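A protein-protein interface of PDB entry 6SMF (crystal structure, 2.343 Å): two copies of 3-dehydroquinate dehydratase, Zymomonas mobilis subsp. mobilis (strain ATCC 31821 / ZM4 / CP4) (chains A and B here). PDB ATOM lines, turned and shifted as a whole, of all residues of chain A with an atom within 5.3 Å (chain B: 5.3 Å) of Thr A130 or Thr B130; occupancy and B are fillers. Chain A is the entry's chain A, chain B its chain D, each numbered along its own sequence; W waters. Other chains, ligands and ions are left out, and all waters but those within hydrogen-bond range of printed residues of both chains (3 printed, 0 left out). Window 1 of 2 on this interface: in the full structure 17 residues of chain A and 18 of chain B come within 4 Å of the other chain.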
ATOM      1  N   ILE A 104      -0.155 -26.620  20.738  1.00  0.00           N
ATOM      2  CA  ILE A 104      -0.452 -25.814  21.951  1.00  0.00           C
ATOM      3  C   ILE A 104      -1.344 -24.628  21.558  1.00  0.00           C
ATOM      4  O   ILE A 104      -0.942 -23.815  20.669  1.00  0.00           O
ATOM      5  CB  ILE A 104       0.850 -25.357  22.598  1.00  0.00           C
ATOM      6  CG1 ILE A 104       1.675 -26.559  23.026  1.00  0.00           C
ATOM      7  CG2 ILE A 104       0.552 -24.430  23.761  1.00  0.00           C
ATOM      8  CD1 ILE A 104       3.098 -26.196  23.346  1.00  0.00           C
ATOM      9  N   GLU A 105      -2.523 -24.555  22.170  1.00  0.00           N
ATOM     10  CA  GLU A 105      -3.453 -23.422  21.986  1.00  0.00           C
ATOM     11  C   GLU A 105      -2.893 -22.244  22.773  1.00  0.00           C
ATOM     12  O   GLU A 105      -2.519 -22.441  23.930  1.00  0.00           O
ATOM     13  CB  GLU A 105      -4.842 -23.776  22.502  1.00  0.00           C
ATOM     14  CG  GLU A 105      -5.907 -22.786  22.106  1.00  0.00           C
ATOM     15  CD  GLU A 105      -7.296 -23.118  22.649  1.00  0.00           C
ATOM     16  OE1 GLU A 105      -7.447 -24.112  23.478  1.00  0.00           O
ATOM     17  OE2 GLU A 105      -8.243 -22.375  22.241  1.00  0.00           O
ATOM     18  N   HIS A 107      -3.858 -17.969  23.636  1.00  0.00           N
ATOM     19  CA  HIS A 107      -4.629 -16.710  23.593  1.00  0.00           C
ATOM     20  C   HIS A 107      -3.898 -15.669  24.448  1.00  0.00           C
ATOM     21  O   HIS A 107      -3.458 -15.990  25.567  1.00  0.00           O
ATOM     22  CB  HIS A 107      -6.087 -16.880  24.068  1.00  0.00           C
ATOM     23  CG  HIS A 107      -6.774 -18.023  23.406  1.00  0.00           C
ATOM     24  ND1 HIS A 107      -7.164 -17.983  22.090  1.00  0.00           N
ATOM     25  CD2 HIS A 107      -7.110 -19.247  23.877  1.00  0.00           C
ATOM     26  CE1 HIS A 107      -7.761 -19.110  21.798  1.00  0.00           C
ATOM     27  NE2 HIS A 107      -7.724 -19.910  22.886  1.00  0.00           N
ATOM     28  N   ASN A 110      -7.940 -13.984  28.197  1.00  0.00           N
ATOM     29  CA  ASN A 110      -8.599 -15.190  28.732  1.00  0.00           C
ATOM     30  C   ASN A 110      -9.979 -15.251  28.088  1.00  0.00           C
ATOM     31  O   ASN A 110     -10.877 -14.489  28.456  1.00  0.00           O
ATOM     32  CB  ASN A 110      -8.645 -15.134  30.264  1.00  0.00           C
ATOM     33  CG  ASN A 110      -9.436 -16.261  30.902  1.00  0.00           C
ATOM     34  OD1 ASN A 110      -9.929 -17.171  30.221  1.00  0.00           O
ATOM     35  ND2 ASN A 110      -9.556 -16.189  32.223  1.00  0.00           N
ATOM     36  N   GLY A 124      -8.941 -26.166  21.444  1.00  0.00           N
ATOM     37  CA  GLY A 124      -8.748 -26.762  22.776  1.00  0.00           C
ATOM     38  C   GLY A 124      -9.256 -28.190  22.853  1.00  0.00           C
ATOM     39  O   GLY A 124      -8.705 -28.970  23.634  1.00  0.00           O
ATOM     40  N   ALA A 127      -6.255 -30.060  20.895  1.00  0.00           N
ATOM     41  CA  ALA A 127      -4.871 -29.712  21.206  1.00  0.00           C
ATOM     42  C   ALA A 127      -4.393 -30.484  22.426  1.00  0.00           C
ATOM     43  O   ALA A 127      -5.189 -31.090  23.137  1.00  0.00           O
ATOM     44  CB  ALA A 127      -4.750 -28.231  21.423  1.00  0.00           C
ATOM     45  N   LEU A 128      -3.079 -30.485  22.594  1.00  0.00           N
ATOM     46  CA  LEU A 128      -2.396 -31.084  23.736  1.00  0.00           C
ATOM     47  C   LEU A 128      -2.783 -30.266  24.960  1.00  0.00           C
ATOM     48  O   LEU A 128      -3.032 -30.813  26.051  1.00  0.00           O
ATOM     49  CB  LEU A 128      -0.892 -31.001  23.469  1.00  0.00           C
ATOM     50  CG  LEU A 128       0.017 -31.419  24.615  1.00  0.00           C
ATOM     51  CD1 LEU A 128      -0.036 -32.919  24.824  1.00  0.00           C
ATOM     52  CD2 LEU A 128       1.446 -30.957  24.332  1.00  0.00           C
ATOM     53  N   GLY A 129      -2.749 -28.959  24.797  1.00  0.00           N
ATOM     54  CA  GLY A 129      -2.738 -28.032  25.941  1.00  0.00           C
ATOM     55  C   GLY A 129      -3.041 -26.630  25.476  1.00  0.00           C
ATOM     56  O   GLY A 129      -3.011 -26.423  24.244  1.00  0.00           O
ATOM     57  N   THR A 130      -3.278 -25.740  26.446  1.00  0.00           N
ATOM     58  CA  THR A 130      -3.782 -24.370  26.265  1.00  0.00           C
ATOM     59  C   THR A 130      -3.078 -23.452  27.255  1.00  0.00           C
ATOM     60  O   THR A 130      -3.045 -23.760  28.458  1.00  0.00           O
ATOM     61  CB  THR A 130      -5.299 -24.331  26.500  1.00  0.00           C
ATOM     62  OG1 THR A 130      -5.895 -25.173  25.511  1.00  0.00           O
ATOM     63  CG2 THR A 130      -5.897 -22.948  26.389  1.00  0.00           C
ATOM     64  N   ILE A 131      -2.600 -22.318  26.751  1.00  0.00           N
ATOM     65  CA  ILE A 131      -2.082 -21.202  27.580  1.00  0.00           C
ATOM     66  C   ILE A 131      -2.846 -19.946  27.180  1.00  0.00           C
ATOM     67  O   ILE A 131      -2.771 -19.552  26.015  1.00  0.00           O
ATOM     68  CB  ILE A 131      -0.578 -21.072  27.413  1.00  0.00           C
ATOM     69  CG1 ILE A 131       0.103 -22.416  27.699  1.00  0.00           C
ATOM     70  CG2 ILE A 131      -0.081 -19.933  28.303  1.00  0.00           C
ATOM     71  CD1 ILE A 131       1.641 -22.408  27.595  1.00  0.00           C
ATOM     72  N   SER A 132      -3.567 -19.370  28.133  1.00  0.00           N
ATOM     73  CA  SER A 132      -4.444 -18.203  27.911  1.00  0.00           C
ATOM     74  C   SER A 132      -4.174 -17.125  28.945  1.00  0.00           C
ATOM     75  O   SER A 132      -4.129 -17.469  30.114  1.00  0.00           O
ATOM     76  CB  SER A 132      -5.901 -18.607  27.980  1.00  0.00           C
ATOM     77  OG  SER A 132      -6.215 -19.414  26.872  1.00  0.00           O
ATOM     78  N   GLY A 133      -4.145 -15.867  28.506  1.00  0.00           N
ATOM     79  CA  GLY A 133      -4.501 -14.717  29.357  1.00  0.00           C
ATOM     80  C   GLY A 133      -3.309 -13.911  29.784  1.00  0.00           C
ATOM     81  O   GLY A 133      -3.534 -12.963  30.532  1.00  0.00           O
ATOM     82  N   PHE A 134      -2.104 -14.253  29.304  1.00  0.00           N
ATOM     83  CA  PHE A 134      -0.833 -13.647  29.786  1.00  0.00           C
ATOM     84  C   PHE A 134      -0.276 -12.663  28.743  1.00  0.00           C
ATOM     85  O   PHE A 134       0.919 -12.339  28.818  1.00  0.00           O
ATOM     86  CB  PHE A 134       0.195 -14.739  30.121  1.00  0.00           C
ATOM     87  CG  PHE A 134      -0.287 -15.762  31.117  1.00  0.00           C
ATOM     88  CD1 PHE A 134      -0.237 -15.510  32.478  1.00  0.00           C
ATOM     89  CD2 PHE A 134      -0.863 -16.959  30.686  1.00  0.00           C
ATOM     90  CE1 PHE A 134      -0.726 -16.444  33.384  1.00  0.00           C
ATOM     91  CE2 PHE A 134      -1.313 -17.904  31.598  1.00  0.00           C
ATOM     92  CZ  PHE A 134      -1.240 -17.642  32.941  1.00  0.00           C
ATOM     93  N   ILE B 104      -4.172 -17.967  38.703  1.00  0.00           N
ATOM     94  CA  ILE B 104      -3.874 -18.775  37.493  1.00  0.00           C
ATOM     95  C   ILE B 104      -4.571 -20.136  37.629  1.00  0.00           C
ATOM     96  O   ILE B 104      -4.309 -20.862  38.611  1.00  0.00           O
ATOM     97  CB  ILE B 104      -2.362 -18.894  37.299  1.00  0.00           C
ATOM     98  CG1 ILE B 104      -1.774 -17.521  37.038  1.00  0.00           C
ATOM     99  CG2 ILE B 104      -2.034 -19.864  36.185  1.00  0.00           C
ATOM    100  CD1 ILE B 104      -0.283 -17.495  37.167  1.00  0.00           C
ATOM    101  N   GLU B 105      -5.429 -20.452  36.668  1.00  0.00           N
ATOM    102  CA  GLU B 105      -6.082 -21.763  36.590  1.00  0.00           C
ATOM    103  C   GLU B 105      -5.062 -22.759  36.066  1.00  0.00           C
ATOM    104  O   GLU B 105      -4.399 -22.448  35.085  1.00  0.00           O
ATOM    105  CB  GLU B 105      -7.302 -21.696  35.689  1.00  0.00           C
ATOM    106  CG  GLU B 105      -8.195 -22.921  35.756  1.00  0.00           C
ATOM    107  CD  GLU B 105      -9.385 -22.869  34.800  1.00  0.00           C
ATOM    108  OE1 GLU B 105      -9.463 -21.924  33.975  1.00  0.00           O
ATOM    109  OE2 GLU B 105     -10.235 -23.803  34.847  1.00  0.00           O
ATOM    110  N   HIS B 107      -4.739 -27.096  35.093  1.00  0.00           N
ATOM    111  CA  HIS B 107      -5.185 -28.497  34.912  1.00  0.00           C
ATOM    112  C   HIS B 107      -4.012 -29.324  34.378  1.00  0.00           C
ATOM    113  O   HIS B 107      -3.336 -28.877  33.451  1.00  0.00           O
ATOM    114  CB  HIS B 107      -6.405 -28.604  33.987  1.00  0.00           C
ATOM    115  CG  HIS B 107      -7.502 -27.685  34.364  1.00  0.00           C
ATOM    116  ND1 HIS B 107      -8.308 -27.914  35.446  1.00  0.00           N
ATOM    117  CD2 HIS B 107      -7.947 -26.538  33.794  1.00  0.00           C
ATOM    118  CE1 HIS B 107      -9.189 -26.936  35.539  1.00  0.00           C
ATOM    119  NE2 HIS B 107      -8.991 -26.081  34.524  1.00  0.00           N
ATOM    120  N   ASN B 110      -6.164 -31.695  29.612  1.00  0.00           N
ATOM    121  CA  ASN B 110      -6.865 -30.632  28.846  1.00  0.00           C
ATOM    122  C   ASN B 110      -8.362 -30.900  29.016  1.00  0.00           C
ATOM    123  O   ASN B 110      -8.895 -31.833  28.416  1.00  0.00           O
ATOM    124  CB  ASN B 110      -6.392 -30.621  27.385  1.00  0.00           C
ATOM    125  CG  ASN B 110      -7.194 -29.675  26.504  1.00  0.00           C
ATOM    126  OD1 ASN B 110      -8.088 -28.911  26.965  1.00  0.00           O
ATOM    127  ND2 ASN B 110      -6.896 -29.729  25.217  1.00  0.00           N
ATOM    128  N   GLY B 124     -11.970 -20.292  35.323  1.00  0.00           N
ATOM    129  CA  GLY B 124     -11.484 -19.626  34.105  1.00  0.00           C
ATOM    130  C   GLY B 124     -12.252 -18.343  33.811  1.00  0.00           C
ATOM    131  O   GLY B 124     -11.646 -17.423  33.232  1.00  0.00           O
ATOM    132  N   ALA B 127     -10.475 -15.901  36.483  1.00  0.00           N
ATOM    133  CA  ALA B 127      -9.004 -15.940  36.619  1.00  0.00           C
ATOM    134  C   ALA B 127      -8.336 -15.028  35.589  1.00  0.00           C
ATOM    135  O   ALA B 127      -8.985 -14.546  34.638  1.00  0.00           O
ATOM    136  CB  ALA B 127      -8.514 -17.357  36.455  1.00  0.00           C
ATOM    137  N   LEU B 128      -7.077 -14.758  35.834  1.00  0.00           N
ATOM    138  CA  LEU B 128      -6.210 -13.960  34.939  1.00  0.00           C
ATOM    139  C   LEU B 128      -6.026 -14.784  33.667  1.00  0.00           C
ATOM    140  O   LEU B 128      -6.101 -14.198  32.552  1.00  0.00           O
ATOM    141  CB  LEU B 128      -4.865 -13.731  35.637  1.00  0.00           C
ATOM    142  CG  LEU B 128      -3.778 -13.073  34.787  1.00  0.00           C
ATOM    143  CD1 LEU B 128      -4.060 -11.621  34.474  1.00  0.00           C
ATOM    144  CD2 LEU B 128      -2.458 -13.151  35.529  1.00  0.00           C
ATOM    145  N   GLY B 129      -5.729 -16.067  33.889  1.00  0.00           N
ATOM    146  CA  GLY B 129      -5.204 -16.963  32.863  1.00  0.00           C
ATOM    147  C   GLY B 129      -5.339 -18.416  33.277  1.00  0.00           C
ATOM    148  O   GLY B 129      -5.593 -18.662  34.462  1.00  0.00           O
ATOM    149  N   THR B 130      -5.078 -19.314  32.324  1.00  0.00           N
ATOM    150  CA  THR B 130      -5.260 -20.769  32.418  1.00  0.00           C
ATOM    151  C   THR B 130      -4.084 -21.461  31.716  1.00  0.00           C
ATOM    152  O   THR B 130      -3.756 -21.106  30.577  1.00  0.00           O
ATOM    153  CB  THR B 130      -6.576 -21.171  31.748  1.00  0.00           C
ATOM    154  OG1 THR B 130      -7.631 -20.486  32.418  1.00  0.00           O
ATOM    155  CG2 THR B 130      -6.831 -22.656  31.757  1.00  0.00           C
ATOM    156  N   ILE B 131      -3.513 -22.461  32.371  1.00  0.00           N
ATOM    157  CA  ILE B 131      -2.584 -23.429  31.765  1.00  0.00           C
ATOM    158  C   ILE B 131      -3.147 -24.833  31.958  1.00  0.00           C
ATOM    159  O   ILE B 131      -3.341 -25.238  33.110  1.00  0.00           O
ATOM    160  CB  ILE B 131      -1.205 -23.249  32.381  1.00  0.00           C
ATOM    161  CG1 ILE B 131      -0.752 -21.789  32.269  1.00  0.00           C
ATOM    162  CG2 ILE B 131      -0.238 -24.227  31.718  1.00  0.00           C
ATOM    163  CD1 ILE B 131       0.534 -21.494  32.945  1.00  0.00           C
ATOM    164  N   SER B 132      -3.383 -25.533  30.854  1.00  0.00           N
ATOM    165  CA  SER B 132      -3.978 -26.867  30.839  1.00  0.00           C
ATOM    166  C   SER B 132      -3.163 -27.816  29.981  1.00  0.00           C
ATOM    167  O   SER B 132      -2.842 -27.434  28.846  1.00  0.00           O
ATOM    168  CB  SER B 132      -5.378 -26.803  30.290  1.00  0.00           C
ATOM    169  OG  SER B 132      -6.228 -26.066  31.158  1.00  0.00           O
ATOM    170  N   GLY B 133      -2.988 -29.055  30.457  1.00  0.00           N
ATOM    171  CA  GLY B 133      -2.804 -30.221  29.578  1.00  0.00           C
ATOM    172  C   GLY B 133      -1.398 -30.729  29.567  1.00  0.00           C
ATOM    173  O   GLY B 133      -1.167 -31.679  28.824  1.00  0.00           O
ATOM    174  N   PHE B 134      -0.506 -30.146  30.369  1.00  0.00           N
ATOM    175  CA  PHE B 134       0.954 -30.471  30.351  1.00  0.00           C
ATOM    176  C   PHE B 134       1.324 -31.337  31.559  1.00  0.00           C
ATOM    177  O   PHE B 134       2.483 -31.397  31.867  1.00  0.00           O
ATOM    178  CB  PHE B 134       1.783 -29.179  30.346  1.00  0.00           C
ATOM    179  CG  PHE B 134       1.457 -28.229  29.223  1.00  0.00           C
ATOM    180  CD1 PHE B 134       2.096 -28.376  28.006  1.00  0.00           C
ATOM    181  CD2 PHE B 134       0.487 -27.235  29.359  1.00  0.00           C
ATOM    182  CE1 PHE B 134       1.770 -27.543  26.941  1.00  0.00           C
ATOM    183  CE2 PHE B 134       0.148 -26.431  28.292  1.00  0.00           C
ATOM    184  CZ  PHE B 134       0.779 -26.590  27.081  1.00  0.00           C
HETATM  185  O   HOH W   1      -9.309 -19.821  30.393  1.00  0.00           O
HETATM  186  O   HOH W   2      -3.040 -33.438  27.933  1.00  0.00           O
HETATM  187  O   HOH W   3      -8.192 -26.241  26.643  1.00  0.00           O
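Among the printed residues, pairs that only touch across the chains: Gly A129 with Ser B132, Ser A132 with Gly B129, Thr A130 with Ile B131, Ile A131 with Thr B130, Asn A110 with Leu B128, Leu A128 with Asn B110, Phe A134 with Ile B104, Thr A130 with Phe B134, Ile A104 with Phe B134, Gly A129 with Phe B134 and Phe A134 with Ile B131.
The backbone carbonyl oxygen (O) of Gly B124 sits at hydrogen-bond distance from the side-chain amide nitrogen (ND2) of Asn A110 (2.6 Å).
O of Gly A133 sits close to O of Leu B128, 3.5 Å away.
O of Thr A130 sits close to O of Thr B130 (3.5 Å).
The backbone NH of Ser A132 is in hydrogen-bond range of the backbone carbonyl oxygen of Thr B130, 3.0 Å away.
The backbone carbonyl oxygen of Leu A128 sits close to the backbone carbonyl oxygen of Gly B133 (3.5 Å).
O of Ala A127 sits at hydrogen-bond distance from ND2 of Asn B110 (3.0 Å).
The backbone carbonyl oxygen (O) of Gly A124 sits at hydrogen-bond distance from the side-chain amide nitrogen (ND2) of Asn B110 (2.5 Å).
The backbone NH (N) of Thr A130 is in hydrogen-bond range of the backbone carbonyl oxygen (O) of Ser B132 (3.0 Å).
The side-chain amide nitrogen (ND2) of Asn A110 is in hydrogen-bond range of the backbone carbonyl oxygen (O) of Ala B127 (3.0 Å).
Printed residues of chain B within 4 Å of Leu A128: Asn B110 (3.6 Å) and Gly B133 (3.5 Å).
Of chain B, only Thr B130 (3.5 Å), Ile B131 (3.4 Å), Ser B132 (3.0 Å) and Phe B134 (3.95 Å) come within 4 Å of Thr A130.
Of the printed residues of chain B, Ile A131 touches Thr B130.
Glu B105 touches none of the printed residues of chain A.
Thr B130 touches just these residues of chain A: Thr A130 (3.5 Å), Ile A131 (3.4 Å) and Ser A132 (3.0 Å).
Of the printed residues of chain A, Phe B134 touches Ile A104 (3.97 Å), Gly A129 (3.97 Å) and Thr A130 (3.95 Å).
Of the 13 printed residues of chain B, 11 touch a printed residue of chain A.
Printed residues of chain B that touch a printed residue of chain A: Ile B104, Asn B110, Gly B124, Ala B127, Leu B128, Gly B129, Thr B130, Ile B131, Ser B132, Gly B133 and Phe B134.
Of the 13 printed residues of chain A, 11 touch a printed residue of chain B.
Hydrophobic or aromatic side chains of chain A within 4 Å of the printed part of chain B: Ile A104 and Phe A134.
OE1 of Glu B105 sits close to N of Gly B124, 3.3 Å away.
The backbone NH (N) of His B107 is in hydrogen-bond range of the backbone carbonyl oxygen (O) of Ile B131, at 3.1 Å.
The backbone NH of His A107 lies within hydrogen-bond range of the backbone carbonyl oxygen of Ile A131, 3.1 Å away.
The backbone carbonyl oxygen (O) of His B107 sits at hydrogen-bond distance from the backbone NH (N) of Gly B133 (3.0 Å).
N of Glu A105 lies within hydrogen-bond range of O of Gly A129.
The side-chain carboxylate of Glu A105 lies close to the backbone NH of Gly A124, 3.3 Å away.
Water W3 bridges the side-chain amide oxygen of Asn B110 (2.7 Å) and the side-chain hydroxyl of Thr A130 (2.8 Å).
Water W1 lies within hydrogen-bond range of OG1 of Thr B130 (2.7 Å) and OD1 of Asn A110 (2.7 Å).
Water W2 bridges the backbone carbonyl oxygen of Gly B133 (2.7 Å) and the backbone carbonyl oxygen of Leu A128 (3.2 Å).
Gly A129 touches Ser B132, and with the chains exchanged Ser A132 touches Gly B129.
Thr A130 touches Ser B132, and with the chains exchanged Ser A132 touches Thr B130.
Thr A130 touches Phe B134, but with the chains exchanged Phe A134 does not touch Thr B130 (4.1 Å).
Phe A134 touches Ile B131, but with the chains exchanged Ile A131 does not touch Phe B134 (4.1 Å).
Positions printed for both chains: 104, 105, 107, 110, 124, 127, 128, 129, 130, 131, 132, 133 and 134.
Of the 20 pairs that touch across the chains among the printed residues, 17 have their exchanged pair printed and touching as well.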
